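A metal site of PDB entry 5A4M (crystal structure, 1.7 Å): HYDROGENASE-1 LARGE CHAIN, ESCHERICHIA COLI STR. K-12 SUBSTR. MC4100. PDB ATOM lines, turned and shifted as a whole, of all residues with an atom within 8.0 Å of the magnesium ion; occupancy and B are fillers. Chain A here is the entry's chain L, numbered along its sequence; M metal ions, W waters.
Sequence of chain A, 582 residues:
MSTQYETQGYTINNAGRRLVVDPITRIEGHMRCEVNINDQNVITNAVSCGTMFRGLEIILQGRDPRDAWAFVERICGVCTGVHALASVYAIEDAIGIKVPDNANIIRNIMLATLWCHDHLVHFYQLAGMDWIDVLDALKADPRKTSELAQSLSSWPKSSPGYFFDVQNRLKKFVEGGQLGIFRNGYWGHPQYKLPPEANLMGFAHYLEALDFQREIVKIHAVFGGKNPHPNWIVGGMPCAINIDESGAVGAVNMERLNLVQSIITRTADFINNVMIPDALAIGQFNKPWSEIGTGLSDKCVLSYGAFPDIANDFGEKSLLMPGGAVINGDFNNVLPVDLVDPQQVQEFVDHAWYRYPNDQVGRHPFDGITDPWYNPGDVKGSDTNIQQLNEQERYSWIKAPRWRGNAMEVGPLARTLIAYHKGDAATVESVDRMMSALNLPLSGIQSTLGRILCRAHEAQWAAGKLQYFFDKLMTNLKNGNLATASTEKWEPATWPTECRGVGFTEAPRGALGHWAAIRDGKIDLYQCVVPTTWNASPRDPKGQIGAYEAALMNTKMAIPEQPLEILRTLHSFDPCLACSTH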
ATOM      1  N   PHE A  53       2.431  12.111  -0.193  1.00  0.00           N
ATOM      2  CA  PHE A  53       3.742  12.630   0.284  1.00  0.00           C
ATOM      3  C   PHE A  53       4.200  11.766   1.439  1.00  0.00           C
ATOM      4  O   PHE A  53       3.379  11.343   2.288  1.00  0.00           O
ATOM      5  CB  PHE A  53       3.555  14.101   0.728  1.00  0.00           C
ATOM      6  CG  PHE A  53       4.819  14.703   1.338  1.00  0.00           C
ATOM      7  CD1 PHE A  53       5.829  15.133   0.512  1.00  0.00           C
ATOM      8  CD2 PHE A  53       4.926  14.892   2.706  1.00  0.00           C
ATOM      9  CE1 PHE A  53       7.003  15.683   1.067  1.00  0.00           C
ATOM     10  CE2 PHE A  53       6.063  15.445   3.286  1.00  0.00           C
ATOM     11  CZ  PHE A  53       7.085  15.869   2.455  1.00  0.00           C
ATOM     12  N   GLU A  57      13.091  13.666   2.098  1.00  0.00           N
ATOM     13  CA  GLU A  57      14.081  14.706   2.317  1.00  0.00           C
ATOM     14  C   GLU A  57      14.228  15.134   3.798  1.00  0.00           C
ATOM     15  O   GLU A  57      15.299  15.616   4.204  1.00  0.00           O
ATOM     16  CB  GLU A  57      13.772  15.937   1.449  1.00  0.00           C
ATOM     17  CG  GLU A  57      13.837  15.668  -0.015  1.00  0.00           C
ATOM     18  CD  GLU A  57      12.992  16.555  -0.874  1.00  0.00           C
ATOM     19  OE1 GLU A  57      11.923  17.044  -0.406  1.00  0.00           O
ATOM     20  OE2 GLU A  57      13.355  16.697  -2.063  1.00  0.00           O
ATOM     21  N   ILE A  75      12.283   5.611  -2.223  1.00  0.00           N
ATOM     22  CA  ILE A  75      11.412   6.630  -2.898  1.00  0.00           C
ATOM     23  C   ILE A  75      10.548   5.873  -3.864  1.00  0.00           C
ATOM     24  O   ILE A  75       9.382   6.213  -4.073  1.00  0.00           O
ATOM     25  CB  ILE A  75      12.247   7.702  -3.619  1.00  0.00           C
ATOM     26  CG1 ILE A  75      12.833   8.638  -2.536  1.00  0.00           C
ATOM     27  CG2 ILE A  75      11.371   8.431  -4.598  1.00  0.00           C
ATOM     28  CD1 ILE A  75      13.830   9.642  -3.047  1.00  0.00           C
ATOM     29  N   GLU A 347      12.882  25.162  -7.799  1.00  0.00           N
ATOM     30  CA  GLU A 347      11.599  24.666  -7.529  1.00  0.00           C
ATOM     31  C   GLU A 347      10.726  25.727  -6.839  1.00  0.00           C
ATOM     32  O   GLU A 347      11.175  26.387  -5.899  1.00  0.00           O
ATOM     33  CB  GLU A 347      11.657  23.427  -6.637  1.00  0.00           C
ATOM     34  CG  GLU A 347      12.321  22.245  -7.319  1.00  0.00           C
ATOM     35  CD  GLU A 347      12.309  21.029  -6.398  1.00  0.00           C
ATOM     36  OE1 GLU A 347      13.055  21.071  -5.384  1.00  0.00           O
ATOM     37  OE2 GLU A 347      11.603  20.060  -6.767  1.00  0.00           O
ATOM     38  N   TYR A 354       3.390  23.302   0.324  1.00  0.00           N
ATOM     39  CA  TYR A 354       4.653  23.512   1.029  1.00  0.00           C
ATOM     40  C   TYR A 354       4.781  24.984   1.391  1.00  0.00           C
ATOM     41  O   TYR A 354       4.135  25.804   0.749  1.00  0.00           O
ATOM     42  CB  TYR A 354       5.824  23.187   0.147  1.00  0.00           C
ATOM     43  CG  TYR A 354       5.886  21.754  -0.277  1.00  0.00           C
ATOM     44  CD1 TYR A 354       6.302  20.773   0.615  1.00  0.00           C
ATOM     45  CD2 TYR A 354       5.368  21.363  -1.499  1.00  0.00           C
ATOM     46  CE1 TYR A 354       6.323  19.436   0.227  1.00  0.00           C
ATOM     47  CE2 TYR A 354       5.337  20.032  -1.898  1.00  0.00           C
ATOM     48  CZ  TYR A 354       5.810  19.079  -1.037  1.00  0.00           C
ATOM     49  OH  TYR A 354       5.805  17.750  -1.360  1.00  0.00           O
ATOM     50  N   PRO A 365      18.044  23.484  -5.473  1.00  0.00           N
ATOM     51  CA  PRO A 365      17.949  22.484  -4.392  1.00  0.00           C
ATOM     52  C   PRO A 365      18.905  22.597  -3.218  1.00  0.00           C
ATOM     53  O   PRO A 365      18.580  22.143  -2.082  1.00  0.00           O
ATOM     54  CB  PRO A 365      18.193  21.172  -5.157  1.00  0.00           C
ATOM     55  CG  PRO A 365      17.591  21.430  -6.493  1.00  0.00           C
ATOM     56  CD  PRO A 365      18.043  22.854  -6.793  1.00  0.00           C
ATOM     57  N   GLY A 368      17.026  24.316  -0.904  1.00  0.00           N
ATOM     58  CA  GLY A 368      15.702  23.785  -0.923  1.00  0.00           C
ATOM     59  C   GLY A 368      15.087  23.693   0.458  1.00  0.00           C
ATOM     60  O   GLY A 368      15.784  23.663   1.474  1.00  0.00           O
ATOM     61  N   ILE A 369      13.779  23.727   0.505  1.00  0.00           N
ATOM     62  CA  ILE A 369      13.027  23.631   1.787  1.00  0.00           C
ATOM     63  C   ILE A 369      11.875  22.681   1.544  1.00  0.00           C
ATOM     64  O   ILE A 369      11.138  22.829   0.565  1.00  0.00           O
ATOM     65  CB  ILE A 369      12.438  24.996   2.262  1.00  0.00           C
ATOM     66  CG1 ILE A 369      13.559  26.036   2.397  1.00  0.00           C
ATOM     67  CG2 ILE A 369      11.587  24.794   3.521  1.00  0.00           C
ATOM     68  CD1 ILE A 369      13.043  27.440   2.673  1.00  0.00           C
ATOM     69  N   THR A 370      11.716  21.709   2.448  1.00  0.00           N
ATOM     70  CA  THR A 370      10.577  20.806   2.398  1.00  0.00           C
ATOM     71  C   THR A 370       9.800  20.877   3.717  1.00  0.00           C
ATOM     72  O   THR A 370      10.063  20.164   4.671  1.00  0.00           O
ATOM     73  CB  THR A 370      11.056  19.374   2.047  1.00  0.00           C
ATOM     74  OG1 THR A 370      11.755  19.418   0.813  1.00  0.00           O
ATOM     75  CG2 THR A 370       9.843  18.433   1.904  1.00  0.00           C
ATOM     76  N   TRP A 397       0.916  17.878  -3.986  1.00  0.00           N
ATOM     77  CA  TRP A 397       2.096  17.567  -3.219  1.00  0.00           C
ATOM     78  C   TRP A 397       3.374  17.593  -4.047  1.00  0.00           C
ATOM     79  O   TRP A 397       4.476  17.311  -3.527  1.00  0.00           O
ATOM     80  CB  TRP A 397       1.963  16.194  -2.512  1.00  0.00           C
ATOM     81  CG  TRP A 397       1.004  16.189  -1.376  1.00  0.00           C
ATOM     82  CD1 TRP A 397      -0.165  15.598  -1.322  1.00  0.00           C
ATOM     83  CD2 TRP A 397       1.164  16.906  -0.145  1.00  0.00           C
ATOM     84  NE1 TRP A 397      -0.759  15.823  -0.105  1.00  0.00           N
ATOM     85  CE2 TRP A 397       0.045  16.642   0.643  1.00  0.00           C
ATOM     86  CE3 TRP A 397       2.207  17.687   0.386  1.00  0.00           C
ATOM     87  CZ2 TRP A 397      -0.151  17.172   1.901  1.00  0.00           C
ATOM     88  CZ3 TRP A 397       2.012  18.234   1.668  1.00  0.00           C
ATOM     89  CH2 TRP A 397       0.853  17.921   2.413  1.00  0.00           C
ATOM     90  N   ILE A 398       3.278  17.912  -5.341  1.00  0.00           N
ATOM     91  CA  ILE A 398       4.452  17.955  -6.213  1.00  0.00           C
ATOM     92  C   ILE A 398       4.956  19.396  -6.316  1.00  0.00           C
ATOM     93  O   ILE A 398       4.209  20.284  -6.609  1.00  0.00           O
ATOM     94  CB  ILE A 398       4.124  17.404  -7.579  1.00  0.00           C
ATOM     95  CG1 ILE A 398       3.499  16.004  -7.510  1.00  0.00           C
ATOM     96  CG2 ILE A 398       5.348  17.403  -8.464  1.00  0.00           C
ATOM     97  CD1 ILE A 398       2.968  15.497  -8.813  1.00  0.00           C
ATOM     98  N   LYS A 399       6.244  19.616  -6.041  1.00  0.00           N
ATOM     99  CA  LYS A 399       6.871  20.910  -6.303  1.00  0.00           C
ATOM    100  C   LYS A 399       6.945  21.189  -7.775  1.00  0.00           C
ATOM    101  O   LYS A 399       6.833  20.292  -8.578  1.00  0.00           O
ATOM    102  CB  LYS A 399       8.251  21.044  -5.651  1.00  0.00           C
ATOM    103  CG  LYS A 399       8.297  20.877  -4.151  1.00  0.00           C
ATOM    104  CD  LYS A 399       9.717  21.116  -3.613  1.00  0.00           C
ATOM    105  CE  LYS A 399       9.882  20.992  -2.114  1.00  0.00           C
ATOM    106  NZ  LYS A 399      11.303  20.880  -1.748  1.00  0.00           N
ATOM    107  N   PRO A 401       9.407  22.280 -10.544  1.00  0.00           N
ATOM    108  CA  PRO A 401      10.748  22.620 -11.034  1.00  0.00           C
ATOM    109  C   PRO A 401      10.690  23.359 -12.348  1.00  0.00           C
ATOM    110  O   PRO A 401       9.820  23.081 -13.194  1.00  0.00           O
ATOM    111  CB  PRO A 401      11.426  21.244 -11.275  1.00  0.00           C
ATOM    112  CG  PRO A 401      10.463  20.229 -10.714  1.00  0.00           C
ATOM    113  CD  PRO A 401       9.074  20.874 -10.851  1.00  0.00           C
ATOM    114  N   GLY A 513      18.016  14.204 -10.107  1.00  0.00           N
ATOM    115  CA  GLY A 513      19.117  14.787  -9.336  1.00  0.00           C
ATOM    116  C   GLY A 513      18.881  14.675  -7.849  1.00  0.00           C
ATOM    117  O   GLY A 513      17.754  14.819  -7.388  1.00  0.00           O
ATOM    118  N   TRP A 515      20.747  16.406  -4.429  1.00  0.00           N
ATOM    119  CA  TRP A 515      21.670  17.419  -3.916  1.00  0.00           C
ATOM    120  C   TRP A 515      21.858  17.182  -2.457  1.00  0.00           C
ATOM    121  O   TRP A 515      20.859  17.156  -1.718  1.00  0.00           O
ATOM    122  CB  TRP A 515      21.044  18.789  -4.181  1.00  0.00           C
ATOM    123  CG  TRP A 515      21.074  19.271  -5.564  1.00  0.00           C
ATOM    124  CD1 TRP A 515      21.941  20.216  -6.061  1.00  0.00           C
ATOM    125  CD2 TRP A 515      20.190  18.927  -6.658  1.00  0.00           C
ATOM    126  NE1 TRP A 515      21.681  20.428  -7.429  1.00  0.00           N
ATOM    127  CE2 TRP A 515      20.598  19.670  -7.790  1.00  0.00           C
ATOM    128  CE3 TRP A 515      19.101  18.081  -6.788  1.00  0.00           C
ATOM    129  CZ2 TRP A 515      19.930  19.595  -9.011  1.00  0.00           C
ATOM    130  CZ3 TRP A 515      18.448  18.023  -8.013  1.00  0.00           C
ATOM    131  CH2 TRP A 515      18.862  18.767  -9.093  1.00  0.00           C
ATOM    132  N   TYR A 526      19.263  17.217   2.149  1.00  0.00           N
ATOM    133  CA  TYR A 526      19.192  16.258   1.066  1.00  0.00           C
ATOM    134  C   TYR A 526      17.929  16.612   0.314  1.00  0.00           C
ATOM    135  O   TYR A 526      16.833  16.432   0.819  1.00  0.00           O
ATOM    136  CB  TYR A 526      19.097  14.849   1.614  1.00  0.00           C
ATOM    137  CG  TYR A 526      19.546  13.789   0.639  1.00  0.00           C
ATOM    138  CD1 TYR A 526      18.793  13.445  -0.443  1.00  0.00           C
ATOM    139  CD2 TYR A 526      20.789  13.137   0.810  1.00  0.00           C
ATOM    140  CE1 TYR A 526      19.254  12.484  -1.360  1.00  0.00           C
ATOM    141  CE2 TYR A 526      21.234  12.183  -0.110  1.00  0.00           C
ATOM    142  CZ  TYR A 526      20.463  11.871  -1.171  1.00  0.00           C
ATOM    143  OH  TYR A 526      20.947  10.911  -2.054  1.00  0.00           O
ATOM    144  N   GLN A 527      18.079  17.136  -0.876  1.00  0.00           N
ATOM    145  CA  GLN A 527      16.982  17.478  -1.694  1.00  0.00           C
ATOM    146  C   GLN A 527      16.975  16.733  -3.043  1.00  0.00           C
ATOM    147  O   GLN A 527      18.014  16.640  -3.723  1.00  0.00           O
ATOM    148  CB  GLN A 527      16.995  18.994  -1.984  1.00  0.00           C
ATOM    149  CG  GLN A 527      16.614  19.808  -0.735  1.00  0.00           C
ATOM    150  CD  GLN A 527      15.138  19.836  -0.492  1.00  0.00           C
ATOM    151  OE1 GLN A 527      14.371  19.948  -1.408  1.00  0.00           O
ATOM    152  NE2 GLN A 527      14.741  19.856   0.736  1.00  0.00           N
ATOM    153  N   CYS A 528      15.800  16.242  -3.431  1.00  0.00           N
ATOM    154  CA  CYS A 528      15.644  15.455  -4.638  1.00  0.00           C
ATOM    155  C   CYS A 528      14.711  16.173  -5.563  1.00  0.00           C
ATOM    156  O   CYS A 528      13.680  16.689  -5.151  1.00  0.00           O
ATOM    157  CB  CYS A 528      15.021  14.095  -4.318  1.00  0.00           C
ATOM    158  SG  CYS A 528      16.005  13.112  -3.156  1.00  0.00           S
ATOM    159  N   VAL A 529      15.086  16.197  -6.833  1.00  0.00           N
ATOM    160  CA  VAL A 529      14.183  16.623  -7.904  1.00  0.00           C
ATOM    161  C   VAL A 529      14.155  15.499  -8.912  1.00  0.00           C
ATOM    162  O   VAL A 529      15.187  15.103  -9.465  1.00  0.00           O
ATOM    163  CB  VAL A 529      14.658  17.926  -8.580  1.00  0.00           C
ATOM    164  CG1 VAL A 529      13.600  18.439  -9.561  1.00  0.00           C
ATOM    165  CG2 VAL A 529      14.981  19.003  -7.576  1.00  0.00           C
ATOM    166  N   VAL A 530      12.978  14.936  -9.132  1.00  0.00           N
ATOM    167  CA  VAL A 530      12.845  13.637  -9.779  1.00  0.00           C
ATOM    168  C   VAL A 530      12.065  13.811 -11.073  1.00  0.00           C
ATOM    169  O   VAL A 530      11.398  14.826 -11.279  1.00  0.00           O
ATOM    170  CB  VAL A 530      12.136  12.721  -8.738  1.00  0.00           C
ATOM    171  CG1 VAL A 530      12.069  11.313  -9.140  1.00  0.00           C
ATOM    172  CG2 VAL A 530      12.865  12.757  -7.394  1.00  0.00           C
ATOM    173  N   THR A 533       8.528  14.734 -10.969  1.00  0.00           N
ATOM    174  CA  THR A 533       8.323  16.086 -10.367  1.00  0.00           C
ATOM    175  C   THR A 533       8.267  17.113 -11.516  1.00  0.00           C
ATOM    176  O   THR A 533       7.440  18.012 -11.506  1.00  0.00           O
ATOM    177  CB  THR A 533       9.436  16.464  -9.393  1.00  0.00           C
ATOM    178  OG1 THR A 533       9.801  15.380  -8.512  1.00  0.00           O
ATOM    179  CG2 THR A 533       9.050  17.675  -8.602  1.00  0.00           C
ATOM    180  N   CYS A 579       7.852   8.722  -6.760  1.00  0.00           N
ATOM    181  CA  CYS A 579       9.032   9.468  -7.140  1.00  0.00           C
ATOM    182  C   CYS A 579       8.759  10.962  -7.070  1.00  0.00           C
ATOM    183  O   CYS A 579       9.644  11.731  -6.640  1.00  0.00           O
ATOM    184  CB  CYS A 579       9.476   9.134  -8.588  1.00  0.00           C
ATOM    185  SG  CYS A 579      10.551   7.689  -8.669  1.00  0.00           S
ATOM    186  N   SER A 580       7.653  11.387  -7.651  1.00  0.00           N
ATOM    187  CA  SER A 580       7.466  12.824  -7.858  1.00  0.00           C
ATOM    188  C   SER A 580       7.448  13.620  -6.581  1.00  0.00           C
ATOM    189  O   SER A 580       7.796  14.802  -6.603  1.00  0.00           O
ATOM    190  CB  SER A 580       6.144  13.101  -8.648  1.00  0.00           C
ATOM    191  OG  SER A 580       4.989  12.890  -7.863  1.00  0.00           O
ATOM    192  N   THR A 581       6.951  12.985  -5.535  1.00  0.00           N
ATOM    193  CA  THR A 581       6.685  13.618  -4.217  1.00  0.00           C
ATOM    194  C   THR A 581       7.692  13.286  -3.157  1.00  0.00           C
ATOM    195  O   THR A 581       8.085  14.123  -2.320  1.00  0.00           O
ATOM    196  CB  THR A 581       5.289  13.216  -3.732  1.00  0.00           C
ATOM    197  OG1 THR A 581       5.153  11.795  -3.762  1.00  0.00           O
ATOM    198  CG2 THR A 581       4.165  13.831  -4.645  1.00  0.00           C
ATOM    199  N   HIS A 582       8.156  12.031  -3.172  1.00  0.00           N
ATOM    200  CA  HIS A 582       9.189  11.578  -2.252  1.00  0.00           C
ATOM    201  C   HIS A 582       8.960  12.089  -0.820  1.00  0.00           C
ATOM    202  O   HIS A 582       9.860  12.488  -0.126  1.00  0.00           O
ATOM    203  CB  HIS A 582      10.596  11.816  -2.811  1.00  0.00           C
ATOM    204  CG  HIS A 582      10.809  13.166  -3.389  1.00  0.00           C
ATOM    205  ND1 HIS A 582      10.493  13.461  -4.684  1.00  0.00           N
ATOM    206  CD2 HIS A 582      11.394  14.280  -2.895  1.00  0.00           C
ATOM    207  CE1 HIS A 582      10.836  14.710  -4.956  1.00  0.00           C
ATOM    208  NE2 HIS A 582      11.349  15.231  -3.882  1.00  0.00           N
ATOM    209  OXT HIS A 582       7.790  11.945  -0.347  1.00  0.00           O
HETATM  210 MG    MG M   1      12.160  17.328  -3.767  1.00  0.00          MG
HETATM  211  O   HOH W   1      11.069  17.882  -5.401  1.00  0.00           O
HETATM  212  O   HOH W   2      10.611  17.897  -2.454  1.00  0.00           O
HETATM  213  O   HOH W   3      13.085  19.191  -3.589  1.00  0.00           O
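The side-chain carboxylate (OE2) of Glu 57 lies close to the side-chain amide oxygen (OE1) of Gln 527 (3.5 Å).
The side-chain hydroxyl of Thr 370 sits at hydrogen-bond distance from the side-chain carboxylate of Glu 57, 2.7 Å away.
O of Cys 579 lies within hydrogen-bond range of ND1 of His 582, at 2.7 Å.
The magnesium ion is bound by water W1 (2.0 Å), water W3 (2.1 Å), water W2 (2.1 Å), O of Cys 528 (2.2 Å), OE2 of Glu 57 (2.2 Å) and NE2 of His 582 (2.3 Å).
Water W3 lies within hydrogen-bond range of OE1 of Glu 347 (2.6 Å), OE1 of Gln 527 (2.6 Å) and NZ of Lys 399 (3.1 Å).
Water W2 lies within hydrogen-bond range of the side-chain carboxylate (OE1) of Glu 57 and the side-chain amino group (NZ) of Lys 399.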
